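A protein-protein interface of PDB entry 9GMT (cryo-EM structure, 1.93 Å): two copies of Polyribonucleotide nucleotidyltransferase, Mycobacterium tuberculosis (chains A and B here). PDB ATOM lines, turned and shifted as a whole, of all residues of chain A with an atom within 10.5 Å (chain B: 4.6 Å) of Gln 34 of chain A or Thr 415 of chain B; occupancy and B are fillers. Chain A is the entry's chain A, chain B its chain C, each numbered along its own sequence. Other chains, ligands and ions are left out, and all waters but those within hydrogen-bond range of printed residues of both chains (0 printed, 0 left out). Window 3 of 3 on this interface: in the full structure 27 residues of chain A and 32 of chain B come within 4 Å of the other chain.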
ATOM      1  N   THR A  28     -27.294   3.364 -10.651  1.00  0.00           N
ATOM      2  CA  THR A  28     -26.196   2.448 -10.382  1.00  0.00           C
ATOM      3  C   THR A  28     -26.641   1.344  -9.435  1.00  0.00           C
ATOM      4  O   THR A  28     -27.551   1.516  -8.621  1.00  0.00           O
ATOM      5  CB  THR A  28     -24.977   3.169  -9.790  1.00  0.00           C
ATOM      6  OG1 THR A  28     -23.837   2.307  -9.856  1.00  0.00           O
ATOM      7  CG2 THR A  28     -25.221   3.547  -8.345  1.00  0.00           C
ATOM      8  N   GLY A  29     -25.967   0.204  -9.547  1.00  0.00           N
ATOM      9  CA  GLY A  29     -26.170  -0.911  -8.650  1.00  0.00           C
ATOM     10  C   GLY A  29     -27.019  -2.050  -9.168  1.00  0.00           C
ATOM     11  O   GLY A  29     -27.396  -2.916  -8.377  1.00  0.00           O
ATOM     12  N   ARG A  30     -27.319  -2.092 -10.458  1.00  0.00           N
ATOM     13  CA  ARG A  30     -28.188  -3.134 -10.990  1.00  0.00           C
ATOM     14  C   ARG A  30     -27.594  -3.906 -12.158  1.00  0.00           C
ATOM     15  O   ARG A  30     -27.894  -5.089 -12.311  1.00  0.00           O
ATOM     16  CB  ARG A  30     -29.535  -2.526 -11.400  1.00  0.00           C
ATOM     17  CG  ARG A  30     -30.515  -3.510 -11.998  1.00  0.00           C
ATOM     18  CD  ARG A  30     -31.859  -2.850 -12.234  1.00  0.00           C
ATOM     19  NE  ARG A  30     -31.964  -2.256 -13.559  1.00  0.00           N
ATOM     20  CZ  ARG A  30     -32.887  -2.573 -14.456  1.00  0.00           C
ATOM     21  NH1 ARG A  30     -33.812  -3.485 -14.205  1.00  0.00           N
ATOM     22  NH2 ARG A  30     -32.886  -1.955 -15.633  1.00  0.00           N
ATOM     23  N   LEU A  31     -26.752  -3.291 -12.982  1.00  0.00           N
ATOM     24  CA  LEU A  31     -26.171  -3.960 -14.137  1.00  0.00           C
ATOM     25  C   LEU A  31     -24.649  -3.941 -14.071  1.00  0.00           C
ATOM     26  O   LEU A  31     -24.045  -2.994 -13.565  1.00  0.00           O
ATOM     27  CB  LEU A  31     -26.631  -3.310 -15.446  1.00  0.00           C
ATOM     28  CG  LEU A  31     -28.124  -3.284 -15.771  1.00  0.00           C
ATOM     29  CD1 LEU A  31     -28.367  -2.654 -17.129  1.00  0.00           C
ATOM     30  CD2 LEU A  31     -28.709  -4.674 -15.721  1.00  0.00           C
ATOM     31  N   ALA A  32     -24.039  -5.011 -14.583  1.00  0.00           N
ATOM     32  CA  ALA A  32     -22.588  -5.116 -14.762  1.00  0.00           C
ATOM     33  C   ALA A  32     -21.837  -4.949 -13.439  1.00  0.00           C
ATOM     34  O   ALA A  32     -21.004  -4.059 -13.272  1.00  0.00           O
ATOM     35  CB  ALA A  32     -22.098  -4.106 -15.802  1.00  0.00           C
ATOM     36  N   LEU A  33     -22.122  -5.853 -12.507  1.00  0.00           N
ATOM     37  CA  LEU A  33     -21.645  -5.699 -11.139  1.00  0.00           C
ATOM     38  C   LEU A  33     -20.199  -6.135 -10.935  1.00  0.00           C
ATOM     39  O   LEU A  33     -19.653  -5.896  -9.856  1.00  0.00           O
ATOM     40  CB  LEU A  33     -22.553  -6.472 -10.183  1.00  0.00           C
ATOM     41  CG  LEU A  33     -24.030  -6.077 -10.188  1.00  0.00           C
ATOM     42  CD1 LEU A  33     -24.797  -6.872  -9.159  1.00  0.00           C
ATOM     43  CD2 LEU A  33     -24.193  -4.594  -9.933  1.00  0.00           C
ATOM     44  N   GLN A  34     -19.561  -6.758 -11.919  1.00  0.00           N
ATOM     45  CA  GLN A  34     -18.168  -7.150 -11.753  1.00  0.00           C
ATOM     46  C   GLN A  34     -17.182  -6.145 -12.330  1.00  0.00           C
ATOM     47  O   GLN A  34     -15.973  -6.362 -12.224  1.00  0.00           O
ATOM     48  CB  GLN A  34     -17.927  -8.526 -12.376  1.00  0.00           C
ATOM     49  CG  GLN A  34     -18.567  -9.649 -11.588  1.00  0.00           C
ATOM     50  CD  GLN A  34     -18.177 -11.016 -12.090  1.00  0.00           C
ATOM     51  OE1 GLN A  34     -16.996 -11.328 -12.227  1.00  0.00           O
ATOM     52  NE2 GLN A  34     -19.171 -11.841 -12.379  1.00  0.00           N
ATOM     53  N   ALA A  35     -17.657  -5.062 -12.934  1.00  0.00           N
ATOM     54  CA  ALA A  35     -16.761  -4.009 -13.380  1.00  0.00           C
ATOM     55  C   ALA A  35     -16.334  -3.148 -12.198  1.00  0.00           C
ATOM     56  O   ALA A  35     -16.949  -3.168 -11.130  1.00  0.00           O
ATOM     57  CB  ALA A  35     -17.431  -3.146 -14.447  1.00  0.00           C
ATOM     58  N   ALA A  36     -15.255  -2.392 -12.393  1.00  0.00           N
ATOM     59  CA  ALA A  36     -14.833  -1.456 -11.358  1.00  0.00           C
ATOM     60  C   ALA A  36     -15.901  -0.398 -11.112  1.00  0.00           C
ATOM     61  O   ALA A  36     -16.174  -0.043  -9.963  1.00  0.00           O
ATOM     62  CB  ALA A  36     -13.499  -0.814 -11.731  1.00  0.00           C
ATOM     63  N   GLY A  37     -16.523   0.108 -12.171  1.00  0.00           N
ATOM     64  CA  GLY A  37     -17.673   0.987 -12.017  1.00  0.00           C
ATOM     65  C   GLY A  37     -18.602   0.874 -13.202  1.00  0.00           C
ATOM     66  O   GLY A  37     -18.164   0.623 -14.326  1.00  0.00           O
ATOM     67  N   ALA A  38     -19.898   1.070 -12.958  1.00  0.00           N
ATOM     68  CA  ALA A  38     -20.887   0.947 -14.025  1.00  0.00           C
ATOM     69  C   ALA A  38     -22.102   1.820 -13.735  1.00  0.00           C
ATOM     70  O   ALA A  38     -22.595   1.846 -12.610  1.00  0.00           O
ATOM     71  CB  ALA A  38     -21.319  -0.508 -14.210  1.00  0.00           C
ATOM     72  N   VAL A  39     -22.589   2.516 -14.767  1.00  0.00           N
ATOM     73  CA  VAL A  39     -23.706   3.449 -14.634  1.00  0.00           C
ATOM     74  C   VAL A  39     -24.624   3.339 -15.848  1.00  0.00           C
ATOM     75  O   VAL A  39     -24.173   3.143 -16.979  1.00  0.00           O
ATOM     76  CB  VAL A  39     -23.218   4.911 -14.465  1.00  0.00           C
ATOM     77  CG1 VAL A  39     -24.389   5.874 -14.400  1.00  0.00           C
ATOM     78  CG2 VAL A  39     -22.366   5.052 -13.225  1.00  0.00           C
ATOM     79  N   LEU A  50     -25.518   2.394 -21.357  1.00  0.00           N
ATOM     80  CA  LEU A  50     -24.756   1.833 -20.244  1.00  0.00           C
ATOM     81  C   LEU A  50     -23.266   2.096 -20.419  1.00  0.00           C
ATOM     82  O   LEU A  50     -22.741   2.002 -21.529  1.00  0.00           O
ATOM     83  CB  LEU A  50     -24.987   0.321 -20.126  1.00  0.00           C
ATOM     84  CG  LEU A  50     -24.015  -0.485 -19.256  1.00  0.00           C
ATOM     85  CD1 LEU A  50     -24.279  -0.291 -17.773  1.00  0.00           C
ATOM     86  CD2 LEU A  50     -24.049  -1.954 -19.624  1.00  0.00           C
ATOM     87  N   SER A  51     -22.579   2.397 -19.318  1.00  0.00           N
ATOM     88  CA  SER A  51     -21.145   2.657 -19.331  1.00  0.00           C
ATOM     89  C   SER A  51     -20.452   1.879 -18.218  1.00  0.00           C
ATOM     90  O   SER A  51     -20.938   1.839 -17.086  1.00  0.00           O
ATOM     91  CB  SER A  51     -20.857   4.149 -19.174  1.00  0.00           C
ATOM     92  OG  SER A  51     -19.472   4.402 -19.209  1.00  0.00           O
ATOM     93  N   ALA A  52     -19.305   1.278 -18.542  1.00  0.00           N
ATOM     94  CA  ALA A  52     -18.554   0.444 -17.609  1.00  0.00           C
ATOM     95  C   ALA A  52     -17.060   0.730 -17.706  1.00  0.00           C
ATOM     96  O   ALA A  52     -16.524   0.890 -18.804  1.00  0.00           O
ATOM     97  CB  ALA A  52     -18.808  -1.042 -17.874  1.00  0.00           C
ATOM     98  N   THR A  53     -16.390   0.757 -16.553  1.00  0.00           N
ATOM     99  CA  THR A  53     -14.962   1.037 -16.448  1.00  0.00           C
ATOM    100  C   THR A  53     -14.279  -0.048 -15.626  1.00  0.00           C
ATOM    101  O   THR A  53     -14.770  -0.419 -14.553  1.00  0.00           O
ATOM    102  CB  THR A  53     -14.708   2.402 -15.799  1.00  0.00           C
ATOM    103  OG1 THR A  53     -15.319   3.431 -16.581  1.00  0.00           O
ATOM    104  CG2 THR A  53     -13.217   2.675 -15.696  1.00  0.00           C
ATOM    105  N   THR A  54     -13.137  -0.531 -16.124  1.00  0.00           N
ATOM    106  CA  THR A  54     -12.339  -1.559 -15.467  1.00  0.00           C
ATOM    107  C   THR A  54     -10.861  -1.197 -15.563  1.00  0.00           C
ATOM    108  O   THR A  54     -10.441  -0.443 -16.441  1.00  0.00           O
ATOM    109  CB  THR A  54     -12.558  -2.948 -16.088  1.00  0.00           C
ATOM    110  OG1 THR A  54     -12.225  -2.911 -17.479  1.00  0.00           O
ATOM    111  CG2 THR A  54     -13.993  -3.389 -15.939  1.00  0.00           C
ATOM    112  N   ALA A  55     -10.067  -1.757 -14.653  1.00  0.00           N
ATOM    113  CA  ALA A  55      -8.627  -1.540 -14.635  1.00  0.00           C
ATOM    114  C   ALA A  55      -7.905  -2.872 -14.491  1.00  0.00           C
ATOM    115  O   ALA A  55      -8.449  -3.832 -13.945  1.00  0.00           O
ATOM    116  CB  ALA A  55      -8.214  -0.596 -13.504  1.00  0.00           C
ATOM    117  N   SER A  56      -6.671  -2.924 -14.986  1.00  0.00           N
ATOM    118  CA  SER A  56      -5.884  -4.149 -14.934  1.00  0.00           C
ATOM    119  C   SER A  56      -5.196  -4.301 -13.582  1.00  0.00           C
ATOM    120  O   SER A  56      -4.951  -3.325 -12.872  1.00  0.00           O
ATOM    121  CB  SER A  56      -4.845  -4.178 -16.055  1.00  0.00           C
ATOM    122  OG  SER A  56      -3.756  -3.320 -15.776  1.00  0.00           O
ATOM    123  N   LYS A  57      -4.889  -5.552 -13.230  1.00  0.00           N
ATOM    124  CA  LYS A  57      -4.292  -5.842 -11.928  1.00  0.00           C
ATOM    125  C   LYS A  57      -2.889  -5.263 -11.805  1.00  0.00           C
ATOM    126  O   LYS A  57      -2.527  -4.725 -10.754  1.00  0.00           O
ATOM    127  CB  LYS A  57      -4.249  -7.351 -11.691  1.00  0.00           C
ATOM    128  CG  LYS A  57      -5.593  -8.052 -11.690  1.00  0.00           C
ATOM    129  CD  LYS A  57      -6.421  -7.712 -10.464  1.00  0.00           C
ATOM    130  CE  LYS A  57      -7.363  -6.549 -10.731  1.00  0.00           C
ATOM    131  NZ  LYS A  57      -8.256  -6.280  -9.569  1.00  0.00           N
ATOM    132  N   GLN A 121      -9.817   0.867 -19.328  1.00  0.00           N
ATOM    133  CA  GLN A 121     -10.701   0.718 -20.474  1.00  0.00           C
ATOM    134  C   GLN A 121     -12.105   1.175 -20.117  1.00  0.00           C
ATOM    135  O   GLN A 121     -12.612   0.867 -19.037  1.00  0.00           O
ATOM    136  CB  GLN A 121     -10.745  -0.725 -20.980  1.00  0.00           C
ATOM    137  CG  GLN A 121     -11.569  -0.876 -22.245  1.00  0.00           C
ATOM    138  CD  GLN A 121     -11.572  -2.280 -22.799  1.00  0.00           C
ATOM    139  OE1 GLN A 121     -11.490  -3.256 -22.060  1.00  0.00           O
ATOM    140  NE2 GLN A 121     -11.670  -2.389 -24.114  1.00  0.00           N
ATOM    141  N   GLY A 150     -15.707   4.237 -10.141  1.00  0.00           N
ATOM    142  CA  GLY A 150     -14.726   3.166 -10.140  1.00  0.00           C
ATOM    143  C   GLY A 150     -13.675   3.219  -9.047  1.00  0.00           C
ATOM    144  O   GLY A 150     -12.926   2.253  -8.891  1.00  0.00           O
ATOM    145  N   GLU B 375     -24.198 -14.955  -9.747  1.00  0.00           N
ATOM    146  CA  GLU B 375     -23.509 -13.828 -10.357  1.00  0.00           C
ATOM    147  C   GLU B 375     -23.588 -13.835 -11.878  1.00  0.00           C
ATOM    148  O   GLU B 375     -23.017 -12.949 -12.514  1.00  0.00           O
ATOM    149  CB  GLU B 375     -22.043 -13.798  -9.926  1.00  0.00           C
ATOM    150  CG  GLU B 375     -21.824 -13.446  -8.473  1.00  0.00           C
ATOM    151  CD  GLU B 375     -20.435 -13.811  -8.001  1.00  0.00           C
ATOM    152  OE1 GLU B 375     -19.483 -13.067  -8.313  1.00  0.00           O
ATOM    153  OE2 GLU B 375     -20.291 -14.848  -7.324  1.00  0.00           O
ATOM    154  N   PHE B 410     -19.711 -11.403 -25.430  1.00  0.00           N
ATOM    155  CA  PHE B 410     -19.037 -11.670 -24.161  1.00  0.00           C
ATOM    156  C   PHE B 410     -17.963 -10.609 -23.934  1.00  0.00           C
ATOM    157  O   PHE B 410     -16.785 -10.821 -24.247  1.00  0.00           O
ATOM    158  CB  PHE B 410     -18.444 -13.081 -24.156  1.00  0.00           C
ATOM    159  CG  PHE B 410     -17.670 -13.426 -22.918  1.00  0.00           C
ATOM    160  CD1 PHE B 410     -18.313 -13.610 -21.711  1.00  0.00           C
ATOM    161  CD2 PHE B 410     -16.301 -13.597 -22.969  1.00  0.00           C
ATOM    162  CE1 PHE B 410     -17.603 -13.938 -20.578  1.00  0.00           C
ATOM    163  CE2 PHE B 410     -15.588 -13.923 -21.838  1.00  0.00           C
ATOM    164  CZ  PHE B 410     -16.241 -14.093 -20.640  1.00  0.00           C
ATOM    165  N   PRO B 412     -15.214  -7.969 -22.153  1.00  0.00           N
ATOM    166  CA  PRO B 412     -14.215  -8.209 -21.100  1.00  0.00           C
ATOM    167  C   PRO B 412     -14.656  -7.777 -19.712  1.00  0.00           C
ATOM    168  O   PRO B 412     -14.177  -8.350 -18.728  1.00  0.00           O
ATOM    169  CB  PRO B 412     -12.999  -7.400 -21.574  1.00  0.00           C
ATOM    170  CG  PRO B 412     -13.257  -7.097 -23.005  1.00  0.00           C
ATOM    171  CD  PRO B 412     -14.732  -7.015 -23.160  1.00  0.00           C
ATOM    172  N   PHE B 413     -15.538  -6.784 -19.590  1.00  0.00           N
ATOM    173  CA  PHE B 413     -15.910  -6.309 -18.264  1.00  0.00           C
ATOM    174  C   PHE B 413     -16.806  -7.279 -17.504  1.00  0.00           C
ATOM    175  O   PHE B 413     -17.008  -7.086 -16.305  1.00  0.00           O
ATOM    176  CB  PHE B 413     -16.557  -4.914 -18.354  1.00  0.00           C
ATOM    177  CG  PHE B 413     -17.894  -4.870 -19.064  1.00  0.00           C
ATOM    178  CD1 PHE B 413     -19.071  -5.231 -18.422  1.00  0.00           C
ATOM    179  CD2 PHE B 413     -17.973  -4.412 -20.363  1.00  0.00           C
ATOM    180  CE1 PHE B 413     -20.274  -5.176 -19.073  1.00  0.00           C
ATOM    181  CE2 PHE B 413     -19.182  -4.346 -21.017  1.00  0.00           C
ATOM    182  CZ  PHE B 413     -20.334  -4.728 -20.372  1.00  0.00           C
ATOM    183  N   SER B 414     -17.348  -8.307 -18.159  1.00  0.00           N
ATOM    184  CA  SER B 414     -18.237  -9.229 -17.458  1.00  0.00           C
ATOM    185  C   SER B 414     -17.501 -10.015 -16.382  1.00  0.00           C
ATOM    186  O   SER B 414     -18.125 -10.483 -15.427  1.00  0.00           O
ATOM    187  CB  SER B 414     -18.906 -10.178 -18.447  1.00  0.00           C
ATOM    188  OG  SER B 414     -17.959 -11.016 -19.063  1.00  0.00           O
ATOM    189  N   THR B 415     -16.189 -10.174 -16.520  1.00  0.00           N
ATOM    190  CA  THR B 415     -15.361 -10.789 -15.497  1.00  0.00           C
ATOM    191  C   THR B 415     -14.513  -9.769 -14.744  1.00  0.00           C
ATOM    192  O   THR B 415     -13.903 -10.113 -13.730  1.00  0.00           O
ATOM    193  CB  THR B 415     -14.473 -11.873 -16.139  1.00  0.00           C
ATOM    194  OG1 THR B 415     -15.309 -12.864 -16.745  1.00  0.00           O
ATOM    195  CG2 THR B 415     -13.611 -12.574 -15.118  1.00  0.00           C
ATOM    196  N   GLY B 416     -14.495  -8.517 -15.181  1.00  0.00           N
ATOM    197  CA  GLY B 416     -13.693  -7.496 -14.549  1.00  0.00           C
ATOM    198  C   GLY B 416     -12.347  -7.241 -15.187  1.00  0.00           C
ATOM    199  O   GLY B 416     -11.460  -6.708 -14.517  1.00  0.00           O
ATOM    200  N   GLU B 417     -12.173  -7.592 -16.454  1.00  0.00           N
ATOM    201  CA  GLU B 417     -10.903  -7.562 -17.162  1.00  0.00           C
ATOM    202  C   GLU B 417     -10.895  -6.420 -18.174  1.00  0.00           C
ATOM    203  O   GLU B 417     -11.909  -5.767 -18.422  1.00  0.00           O
ATOM    204  CB  GLU B 417     -10.665  -8.899 -17.865  1.00  0.00           C
ATOM    205  CG  GLU B 417     -10.479 -10.088 -16.943  1.00  0.00           C
ATOM    206  CD  GLU B 417      -9.215 -10.014 -16.126  1.00  0.00           C
ATOM    207  OE1 GLU B 417      -8.214  -9.451 -16.615  1.00  0.00           O
ATOM    208  OE2 GLU B 417      -9.226 -10.512 -14.982  1.00  0.00           O
ATOM    209  N   GLY B 461     -22.780 -10.254 -16.837  1.00  0.00           N
ATOM    210  CA  GLY B 461     -22.004 -10.828 -15.751  1.00  0.00           C
ATOM    211  C   GLY B 461     -21.893 -12.328 -15.914  1.00  0.00           C
ATOM    212  O   GLY B 461     -22.848 -12.994 -16.308  1.00  0.00           O
ATOM    213  N   SER B 462     -20.723 -12.865 -15.584  1.00  0.00           N
ATOM    214  CA  SER B 462     -20.492 -14.281 -15.840  1.00  0.00           C
ATOM    215  C   SER B 462     -19.736 -14.935 -14.694  1.00  0.00           C
ATOM    216  O   SER B 462     -18.661 -14.472 -14.307  1.00  0.00           O
ATOM    217  CB  SER B 462     -19.727 -14.483 -17.150  1.00  0.00           C
ATOM    218  OG  SER B 462     -18.415 -13.973 -17.055  1.00  0.00           O
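Hydrophobic or aromatic side chains of chain A within 4 Å of the printed part of chain B: Ala 32.
Hydrophobic or aromatic side chains of chain B that line the printed part of chain A: Phe 413.
Among the printed residues, 8 pairs touch across the chains.
Among the printed residues, no Asp or Glu carboxylate lies within 4 Å of a Lys or Arg side-chain nitrogen of the other chain.
Printed residues of chain B within 4 Å of Gln 34 of chain A: Ser 414 (3.4 Å), Thr 415 (3.6 Å), Gly 416 (3.4 Å) and Ser 462 (3.3 Å).
Thr 415 of chain B touches just one residue of chain A: Gln 34.
Ser 414 of chain B touches one residue of chain A.
No residue of chain A comes within 4 Å of Gly 461 of chain B.
Of chain A, only Gln 34 comes within 4 Å of Ser 462 of chain B.
Of the printed residues of chain A, Phe 413 of chain B touches Ala 32 (3.9 Å), Ala 35 (3.99 Å) and Thr 54 (3.8 Å).
Of the printed residues of chain B, Ala 32 of chain A touches Phe 413 (3.9 Å).
Of the printed residues of chain B, Thr 54 of chain A touches Phe 413 and Glu 417.
The nearest printed residue of chain B that does not touch Ala 35 of chain A is Gly 416 of chain B (4.8 Å).
The backbone NH (N) of Gln 121 of chain A is in hydrogen-bond range of the backbone carbonyl oxygen (O) of Thr 54 of chain A, at 3.2 Å.
O of Pro 412 of chain B is in hydrogen-bond range of N of Glu 417 of chain B.
OG1 of Thr 415 of chain B is in hydrogen-bond range of OG of Ser 462 of chain B, at 3.3 Å.
The side-chain amide nitrogen (NE2) of Gln 34 of chain A lies close to the backbone carbonyl oxygen (O) of Ser 414 of chain B (3.5 Å).
The backbone carbonyl oxygen of Ser 462 of chain B lies within hydrogen-bond range of the side-chain amide nitrogen of Gln 34 of chain A.
O of Glu 417 of chain B sits at hydrogen-bond distance from OG1 of Thr 54 of chain A (3.0 Å).
No position is printed for both chains.
Of the 8 pairs that touch across the chains among the printed residues, none has its exchanged pair printed and touching as well.
Among the printed residues, pairs that only touch across the chains: Ala 32 of chain A with Phe 413 of chain B (3.9 Å), Gln 34 of chain A with Thr 415 of chain B (3.6 Å), Gln 34 of chain A with Gly 416 of chain B (3.4 Å), Ala 35 of chain A with Phe 413 of chain B (3.99 Å) and Thr 54 of chain A with Phe 413 of chain B (3.8 Å).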
